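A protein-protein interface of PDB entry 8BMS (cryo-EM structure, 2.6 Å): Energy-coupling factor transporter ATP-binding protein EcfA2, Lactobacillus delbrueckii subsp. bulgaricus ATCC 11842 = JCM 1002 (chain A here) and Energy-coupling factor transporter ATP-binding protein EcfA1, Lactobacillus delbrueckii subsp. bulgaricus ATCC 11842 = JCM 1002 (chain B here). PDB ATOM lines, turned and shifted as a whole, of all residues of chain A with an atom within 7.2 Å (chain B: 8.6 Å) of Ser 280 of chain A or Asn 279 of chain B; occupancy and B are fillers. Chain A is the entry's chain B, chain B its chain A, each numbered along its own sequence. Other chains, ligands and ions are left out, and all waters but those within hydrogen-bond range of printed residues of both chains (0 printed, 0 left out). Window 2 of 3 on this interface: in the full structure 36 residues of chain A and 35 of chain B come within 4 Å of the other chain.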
ATOM      1  N   LEU A 256      -1.053  17.274  11.765  1.00  0.00           N
ATOM      2  CA  LEU A 256       0.035  16.908  12.664  1.00  0.00           C
ATOM      3  C   LEU A 256      -0.083  15.458  13.113  1.00  0.00           C
ATOM      4  O   LEU A 256       0.921  14.741  13.198  1.00  0.00           O
ATOM      5  CB  LEU A 256       0.047  17.845  13.872  1.00  0.00           C
ATOM      6  CG  LEU A 256       1.409  18.225  14.453  1.00  0.00           C
ATOM      7  CD1 LEU A 256       2.313  18.798  13.376  1.00  0.00           C
ATOM      8  CD2 LEU A 256       1.240  19.210  15.594  1.00  0.00           C
ATOM      9  N   GLY A 260       2.355  11.842  12.398  1.00  0.00           N
ATOM     10  CA  GLY A 260       2.857  11.035  13.497  1.00  0.00           C
ATOM     11  C   GLY A 260       2.918  11.736  14.838  1.00  0.00           C
ATOM     12  O   GLY A 260       3.402  11.131  15.806  1.00  0.00           O
ATOM     13  N   LEU A 261       2.459  12.978  14.960  1.00  0.00           N
ATOM     14  CA  LEU A 261       2.480  13.713  16.221  1.00  0.00           C
ATOM     15  C   LEU A 261       1.054  13.788  16.756  1.00  0.00           C
ATOM     16  O   LEU A 261       0.285  14.675  16.376  1.00  0.00           O
ATOM     17  CB  LEU A 261       3.080  15.104  16.032  1.00  0.00           C
ATOM     18  CG  LEU A 261       3.259  15.931  17.307  1.00  0.00           C
ATOM     19  CD1 LEU A 261       3.876  15.089  18.415  1.00  0.00           C
ATOM     20  CD2 LEU A 261       4.104  17.166  17.035  1.00  0.00           C
ATOM     21  N   LYS A 262       0.707  12.856  17.638  1.00  0.00           N
ATOM     22  CA  LYS A 262      -0.620  12.851  18.236  1.00  0.00           C
ATOM     23  C   LYS A 262      -0.742  13.956  19.278  1.00  0.00           C
ATOM     24  O   LYS A 262       0.195  14.229  20.033  1.00  0.00           O
ATOM     25  CB  LYS A 262      -0.913  11.491  18.869  1.00  0.00           C
ATOM     26  CG  LYS A 262       0.152  11.015  19.844  1.00  0.00           C
ATOM     27  CD  LYS A 262      -0.226   9.681  20.467  1.00  0.00           C
ATOM     28  CE  LYS A 262       0.796   9.250  21.506  1.00  0.00           C
ATOM     29  NZ  LYS A 262       2.057   8.767  20.879  1.00  0.00           N
ATOM     30  N   LEU A 263      -1.910  14.596  19.315  1.00  0.00           N
ATOM     31  CA  LEU A 263      -2.172  15.674  20.249  1.00  0.00           C
ATOM     32  C   LEU A 263      -3.290  15.286  21.210  1.00  0.00           C
ATOM     33  O   LEU A 263      -4.264  14.648  20.800  1.00  0.00           O
ATOM     34  CB  LEU A 263      -2.561  16.965  19.512  1.00  0.00           C
ATOM     35  CG  LEU A 263      -1.606  17.463  18.425  1.00  0.00           C
ATOM     36  CD1 LEU A 263      -2.009  18.852  17.962  1.00  0.00           C
ATOM     37  CD2 LEU A 263      -0.170  17.457  18.923  1.00  0.00           C
ATOM     38  N   PRO A 264      -3.175  15.645  22.488  1.00  0.00           N
ATOM     39  CA  PRO A 264      -4.255  15.341  23.435  1.00  0.00           C
ATOM     40  C   PRO A 264      -5.529  16.096  23.083  1.00  0.00           C
ATOM     41  O   PRO A 264      -5.489  17.243  22.631  1.00  0.00           O
ATOM     42  CB  PRO A 264      -3.684  15.793  24.783  1.00  0.00           C
ATOM     43  CG  PRO A 264      -2.638  16.802  24.433  1.00  0.00           C
ATOM     44  CD  PRO A 264      -2.049  16.341  23.134  1.00  0.00           C
ATOM     45  N   ALA A 274      -1.679  25.497  20.114  1.00  0.00           N
ATOM     46  CA  ALA A 274      -0.309  25.753  20.546  1.00  0.00           C
ATOM     47  C   ALA A 274      -0.005  25.048  21.862  1.00  0.00           C
ATOM     48  O   ALA A 274       1.075  24.468  22.032  1.00  0.00           O
ATOM     49  CB  ALA A 274      -0.073  27.258  20.672  1.00  0.00           C
ATOM     50  N   ASP A 275      -0.948  25.087  22.807  1.00  0.00           N
ATOM     51  CA  ASP A 275      -0.763  24.382  24.072  1.00  0.00           C
ATOM     52  C   ASP A 275      -0.647  22.879  23.852  1.00  0.00           C
ATOM     53  O   ASP A 275       0.192  22.218  24.474  1.00  0.00           O
ATOM     54  CB  ASP A 275      -1.916  24.695  25.025  1.00  0.00           C
ATOM     55  CG  ASP A 275      -1.976  26.159  25.406  1.00  0.00           C
ATOM     56  OD1 ASP A 275      -1.107  26.929  24.947  1.00  0.00           O
ATOM     57  OD2 ASP A 275      -2.891  26.542  26.164  1.00  0.00           O
ATOM     58  N   ALA A 276      -1.485  22.322  22.974  1.00  0.00           N
ATOM     59  CA  ALA A 276      -1.409  20.894  22.682  1.00  0.00           C
ATOM     60  C   ALA A 276      -0.075  20.529  22.043  1.00  0.00           C
ATOM     61  O   ALA A 276       0.515  19.492  22.369  1.00  0.00           O
ATOM     62  CB  ALA A 276      -2.568  20.481  21.776  1.00  0.00           C
ATOM     63  N   ILE A 277       0.415  21.367  21.125  1.00  0.00           N
ATOM     64  CA  ILE A 277       1.701  21.107  20.484  1.00  0.00           C
ATOM     65  C   ILE A 277       2.824  21.138  21.512  1.00  0.00           C
ATOM     66  O   ILE A 277       3.705  20.269  21.519  1.00  0.00           O
ATOM     67  CB  ILE A 277       1.944  22.116  19.347  1.00  0.00           C
ATOM     68  CG1 ILE A 277       1.026  21.820  18.161  1.00  0.00           C
ATOM     69  CG2 ILE A 277       3.398  22.089  18.907  1.00  0.00           C
ATOM     70  CD1 ILE A 277       0.919  22.960  17.175  1.00  0.00           C
ATOM     71  N   LYS A 278       2.813  22.139  22.397  1.00  0.00           N
ATOM     72  CA  LYS A 278       3.847  22.221  23.424  1.00  0.00           C
ATOM     73  C   LYS A 278       3.782  21.027  24.370  1.00  0.00           C
ATOM     74  O   LYS A 278       4.820  20.502  24.790  1.00  0.00           O
ATOM     75  CB  LYS A 278       3.718  23.529  24.202  1.00  0.00           C
ATOM     76  CG  LYS A 278       5.000  23.952  24.903  1.00  0.00           C
ATOM     77  CD  LYS A 278       4.719  24.889  26.065  1.00  0.00           C
ATOM     78  CE  LYS A 278       4.482  24.116  27.351  1.00  0.00           C
ATOM     79  NZ  LYS A 278       4.575  24.996  28.549  1.00  0.00           N
ATOM     80  N   GLN A 279       2.570  20.592  24.723  1.00  0.00           N
ATOM     81  CA  GLN A 279       2.420  19.417  25.575  1.00  0.00           C
ATOM     82  C   GLN A 279       2.961  18.167  24.891  1.00  0.00           C
ATOM     83  O   GLN A 279       3.619  17.336  25.528  1.00  0.00           O
ATOM     84  CB  GLN A 279       0.951  19.232  25.953  1.00  0.00           C
ATOM     85  CG  GLN A 279       0.659  17.966  26.742  1.00  0.00           C
ATOM     86  CD  GLN A 279       0.985  18.110  28.214  1.00  0.00           C
ATOM     87  OE1 GLN A 279       1.126  19.220  28.726  1.00  0.00           O
ATOM     88  NE2 GLN A 279       1.107  16.982  28.905  1.00  0.00           N
ATOM     89  N   SER A 280       2.686  18.015  23.593  1.00  0.00           N
ATOM     90  CA  SER A 280       3.199  16.863  22.857  1.00  0.00           C
ATOM     91  C   SER A 280       4.720  16.888  22.783  1.00  0.00           C
ATOM     92  O   SER A 280       5.374  15.848  22.931  1.00  0.00           O
ATOM     93  CB  SER A 280       2.591  16.824  21.456  1.00  0.00           C
ATOM     94  OG  SER A 280       3.286  17.688  20.575  1.00  0.00           O
ATOM     95  N   LEU A 281       5.303  18.065  22.553  1.00  0.00           N
ATOM     96  CA  LEU A 281       6.755  18.186  22.499  1.00  0.00           C
ATOM     97  C   LEU A 281       7.405  18.115  23.873  1.00  0.00           C
ATOM     98  O   LEU A 281       8.628  17.955  23.953  1.00  0.00           O
ATOM     99  CB  LEU A 281       7.152  19.495  21.814  1.00  0.00           C
ATOM    100  CG  LEU A 281       6.696  19.687  20.367  1.00  0.00           C
ATOM    101  CD1 LEU A 281       6.790  21.150  19.972  1.00  0.00           C
ATOM    102  CD2 LEU A 281       7.516  18.823  19.428  1.00  0.00           C
ATOM    103  N   LYS A 282       6.630  18.229  24.947  1.00  0.00           N
ATOM    104  CA  LYS A 282       7.177  18.198  26.298  1.00  0.00           C
ATOM    105  C   LYS A 282       7.448  16.767  26.749  1.00  0.00           C
ATOM    106  O   LYS A 282       6.860  15.819  26.228  1.00  0.00           O
ATOM    107  CB  LYS A 282       6.222  18.888  27.274  1.00  0.00           C
ATOM    108  CG  LYS A 282       6.795  19.093  28.666  1.00  0.00           C
ATOM    109  CD  LYS A 282       5.768  19.720  29.595  1.00  0.00           C
ATOM    110  CE  LYS A 282       6.309  19.855  31.008  1.00  0.00           C
ATOM    111  NZ  LYS A 282       7.329  20.936  31.107  1.00  0.00           N
ATOM    112  N   LEU B 254       3.900  29.701  19.153  1.00  0.00           N
ATOM    113  CA  LEU B 254       4.856  28.677  19.565  1.00  0.00           C
ATOM    114  C   LEU B 254       6.141  29.306  20.090  1.00  0.00           C
ATOM    115  O   LEU B 254       6.732  28.813  21.059  1.00  0.00           O
ATOM    116  CB  LEU B 254       5.147  27.725  18.407  1.00  0.00           C
ATOM    117  CG  LEU B 254       3.987  26.808  18.014  1.00  0.00           C
ATOM    118  CD1 LEU B 254       4.375  25.903  16.857  1.00  0.00           C
ATOM    119  CD2 LEU B 254       3.521  25.990  19.208  1.00  0.00           C
ATOM    120  N   ILE B 259       8.805  27.236  22.116  1.00  0.00           N
ATOM    121  CA  ILE B 259       9.253  26.430  20.983  1.00  0.00           C
ATOM    122  C   ILE B 259       9.762  27.364  19.894  1.00  0.00           C
ATOM    123  O   ILE B 259       9.006  28.181  19.359  1.00  0.00           O
ATOM    124  CB  ILE B 259       8.123  25.533  20.457  1.00  0.00           C
ATOM    125  CG1 ILE B 259       7.600  24.625  21.571  1.00  0.00           C
ATOM    126  CG2 ILE B 259       8.610  24.703  19.279  1.00  0.00           C
ATOM    127  CD1 ILE B 259       8.629  23.649  22.097  1.00  0.00           C
ATOM    128  N   VAL B 272       4.538  21.460   9.872  1.00  0.00           N
ATOM    129  CA  VAL B 272       4.259  20.106  10.346  1.00  0.00           C
ATOM    130  C   VAL B 272       5.538  19.280  10.374  1.00  0.00           C
ATOM    131  O   VAL B 272       5.819  18.568  11.347  1.00  0.00           O
ATOM    132  CB  VAL B 272       3.175  19.447   9.473  1.00  0.00           C
ATOM    133  CG1 VAL B 272       3.180  17.941   9.660  1.00  0.00           C
ATOM    134  CG2 VAL B 272       1.808  20.023   9.803  1.00  0.00           C
ATOM    135  N   GLN B 273       6.337  19.365   9.308  1.00  0.00           N
ATOM    136  CA  GLN B 273       7.585  18.608   9.259  1.00  0.00           C
ATOM    137  C   GLN B 273       8.571  19.091  10.317  1.00  0.00           C
ATOM    138  O   GLN B 273       9.267  18.280  10.940  1.00  0.00           O
ATOM    139  CB  GLN B 273       8.206  18.695   7.865  1.00  0.00           C
ATOM    140  CG  GLN B 273       7.348  18.099   6.757  1.00  0.00           C
ATOM    141  CD  GLN B 273       6.942  16.660   7.028  1.00  0.00           C
ATOM    142  OE1 GLN B 273       7.689  15.892   7.635  1.00  0.00           O
ATOM    143  NE2 GLN B 273       5.748  16.289   6.577  1.00  0.00           N
ATOM    144  N   SER B 274       8.651  20.407  10.533  1.00  0.00           N
ATOM    145  CA  SER B 274       9.545  20.929  11.562  1.00  0.00           C
ATOM    146  C   SER B 274       9.125  20.458  12.949  1.00  0.00           C
ATOM    147  O   SER B 274       9.971  20.073  13.765  1.00  0.00           O
ATOM    148  CB  SER B 274       9.582  22.454  11.501  1.00  0.00           C
ATOM    149  OG  SER B 274      10.658  22.968  12.266  1.00  0.00           O
ATOM    150  N   LEU B 275       7.820  20.479  13.234  1.00  0.00           N
ATOM    151  CA  LEU B 275       7.341  20.000  14.527  1.00  0.00           C
ATOM    152  C   LEU B 275       7.592  18.507  14.692  1.00  0.00           C
ATOM    153  O   LEU B 275       7.946  18.049  15.785  1.00  0.00           O
ATOM    154  CB  LEU B 275       5.857  20.322  14.689  1.00  0.00           C
ATOM    155  CG  LEU B 275       5.519  21.805  14.845  1.00  0.00           C
ATOM    156  CD1 LEU B 275       4.013  22.019  14.848  1.00  0.00           C
ATOM    157  CD2 LEU B 275       6.149  22.367  16.108  1.00  0.00           C
ATOM    158  N   TRP B 276       7.412  17.732  13.620  1.00  0.00           N
ATOM    159  CA  TRP B 276       7.689  16.300  13.689  1.00  0.00           C
ATOM    160  C   TRP B 276       9.164  16.037  13.963  1.00  0.00           C
ATOM    161  O   TRP B 276       9.509  15.159  14.763  1.00  0.00           O
ATOM    162  CB  TRP B 276       7.249  15.623  12.390  1.00  0.00           C
ATOM    163  CG  TRP B 276       7.798  14.241  12.196  1.00  0.00           C
ATOM    164  CD1 TRP B 276       8.491  13.783  11.114  1.00  0.00           C
ATOM    165  CD2 TRP B 276       7.684  13.131  13.097  1.00  0.00           C
ATOM    166  NE1 TRP B 276       8.826  12.462  11.289  1.00  0.00           N
ATOM    167  CE2 TRP B 276       8.341  12.039  12.499  1.00  0.00           C
ATOM    168  CE3 TRP B 276       7.095  12.958  14.355  1.00  0.00           C
ATOM    169  CZ2 TRP B 276       8.426  10.791  13.113  1.00  0.00           C
ATOM    170  CZ3 TRP B 276       7.182  11.719  14.962  1.00  0.00           C
ATOM    171  CH2 TRP B 276       7.841  10.651  14.340  1.00  0.00           C
ATOM    172  N   GLN B 277      10.052  16.794  13.312  1.00  0.00           N
ATOM    173  CA  GLN B 277      11.480  16.642  13.568  1.00  0.00           C
ATOM    174  C   GLN B 277      11.833  17.044  14.995  1.00  0.00           C
ATOM    175  O   GLN B 277      12.678  16.406  15.634  1.00  0.00           O
ATOM    176  CB  GLN B 277      12.286  17.461  12.561  1.00  0.00           C
ATOM    177  CG  GLN B 277      12.422  16.804  11.198  1.00  0.00           C
ATOM    178  CD  GLN B 277      12.684  17.805  10.090  1.00  0.00           C
ATOM    179  OE1 GLN B 277      12.768  19.009  10.332  1.00  0.00           O
ATOM    180  NE2 GLN B 277      12.816  17.310   8.865  1.00  0.00           N
ATOM    181  N   LEU B 278      11.206  18.106  15.508  1.00  0.00           N
ATOM    182  CA  LEU B 278      11.440  18.507  16.892  1.00  0.00           C
ATOM    183  C   LEU B 278      10.988  17.426  17.863  1.00  0.00           C
ATOM    184  O   LEU B 278      11.663  17.154  18.863  1.00  0.00           O
ATOM    185  CB  LEU B 278      10.724  19.824  17.187  1.00  0.00           C
ATOM    186  CG  LEU B 278      11.352  21.100  16.623  1.00  0.00           C
ATOM    187  CD1 LEU B 278      10.389  22.270  16.756  1.00  0.00           C
ATOM    188  CD2 LEU B 278      12.669  21.405  17.315  1.00  0.00           C
ATOM    189  N   ASN B 279       9.840  16.802  17.589  1.00  0.00           N
ATOM    190  CA  ASN B 279       9.357  15.721  18.440  1.00  0.00           C
ATOM    191  C   ASN B 279      10.244  14.487  18.341  1.00  0.00           C
ATOM    192  O   ASN B 279      10.382  13.743  19.319  1.00  0.00           O
ATOM    193  CB  ASN B 279       7.914  15.372  18.076  1.00  0.00           C
ATOM    194  CG  ASN B 279       7.466  14.048  18.663  1.00  0.00           C
ATOM    195  OD1 ASN B 279       7.478  13.020  17.985  1.00  0.00           O
ATOM    196  ND2 ASN B 279       7.069  14.066  19.930  1.00  0.00           N
ATOM    197  N   SER B 280      10.856  14.255  17.176  1.00  0.00           N
ATOM    198  CA  SER B 280      11.709  13.086  16.996  1.00  0.00           C
ATOM    199  C   SER B 280      12.924  13.104  17.914  1.00  0.00           C
ATOM    200  O   SER B 280      13.485  12.041  18.202  1.00  0.00           O
ATOM    201  CB  SER B 280      12.162  12.985  15.539  1.00  0.00           C
ATOM    202  OG  SER B 280      13.329  13.755  15.313  1.00  0.00           O
ATOM    203  N   LYS B 281      13.345  14.278  18.376  1.00  0.00           N
ATOM    204  CA  LYS B 281      14.484  14.376  19.282  1.00  0.00           C
ATOM    205  C   LYS B 281      14.020  14.469  20.733  1.00  0.00           C
ATOM    206  O   LYS B 281      13.525  15.506  21.172  1.00  0.00           O
ATOM    207  CB  LYS B 281      15.350  15.586  18.928  1.00  0.00           C
ATOM    208  CG  LYS B 281      16.101  15.449  17.615  1.00  0.00           C
ATOM    209  CD  LYS B 281      17.409  16.224  17.645  1.00  0.00           C
ATOM    210  CE  LYS B 281      17.167  17.708  17.862  1.00  0.00           C
ATOM    211  NZ  LYS B 281      16.850  18.412  16.591  1.00  0.00           N
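Among the printed residues, merely in contact across the chains: Leu 256 of chain A with Val 272 of chain B (3.8 Å), Leu 256 of chain A with Leu 275 of chain B (3.9 Å), Gly 260 of chain A with Trp 276 of chain B (3.9 Å), Leu 261 of chain A with Asn 279 of chain B (3.7 Å), Ile 277 of chain A with Leu 254 of chain B (3.9 Å), Ile 277 of chain A with Leu 275 of chain B (3.9 Å), Ser 280 of chain A with Asn 279 of chain B (3.9 Å), Leu 281 of chain A with Ile 259 of chain B (3.8 Å), Leu 281 of chain A with Leu 275 of chain B (3.7 Å) and Leu 281 of chain A with Asn 279 of chain B (3.6 Å).
Of the 12 printed residues of chain B, 6 touch a printed residue of chain A. Hydrophobic or aromatic side chains of chain B within 4 Å of the printed part of chain A: Leu 254, Ile 259, Val 272, Leu 275 and Trp 276. Along chain B the printed residues that touch a printed residue of chain A span positions 254 to 279. Hydrophobic or aromatic side chains of chain A within 4 Å of the printed part of chain B: Leu 256, Leu 261, Ile 277 and Leu 281. Among the printed residues, 10 pairs touch across the chains.
O of Ile 277 of chain A sits at hydrogen-bond distance from OG of Ser 280 of chain A (2.8 Å). The backbone carbonyl oxygen (O) of Leu 254 of chain B lies within hydrogen-bond range of the backbone NH (N) of Ile 259 of chain B, at 2.8 Å. The backbone NH of Leu 261 of chain A lies within hydrogen-bond range of the backbone carbonyl oxygen of Leu 256 of chain A (2.9 Å).
Of the printed residues of chain B, Leu 256 of chain A touches Val 272 (3.8 Å) and Leu 275 (3.9 Å). Asp 275 of chain A touches none of the printed residues of chain B. Ser 280 of chain A touches just one residue of chain B: Asn 279 (3.9 Å). Printed residues of chain A within 4 Å of Ile 259 of chain B: Leu 281. Of the printed residues of chain A, Val 272 of chain B touches Leu 256 (3.8 Å). Of the printed residues of chain A, Trp 276 of chain B touches Gly 260. Asn 279 of chain B touches just these residues of chain A: Leu 261 (3.7 Å), Ser 280 (3.9 Å) and Leu 281 (3.6 Å). The nearest residue of chain A that does not touch Asn 279 of chain B is Gly 260 of chain A (5.0 Å). The nearest printed residue of chain B that does not touch Leu 281 of chain A is Leu 278 of chain B (4.04 Å).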
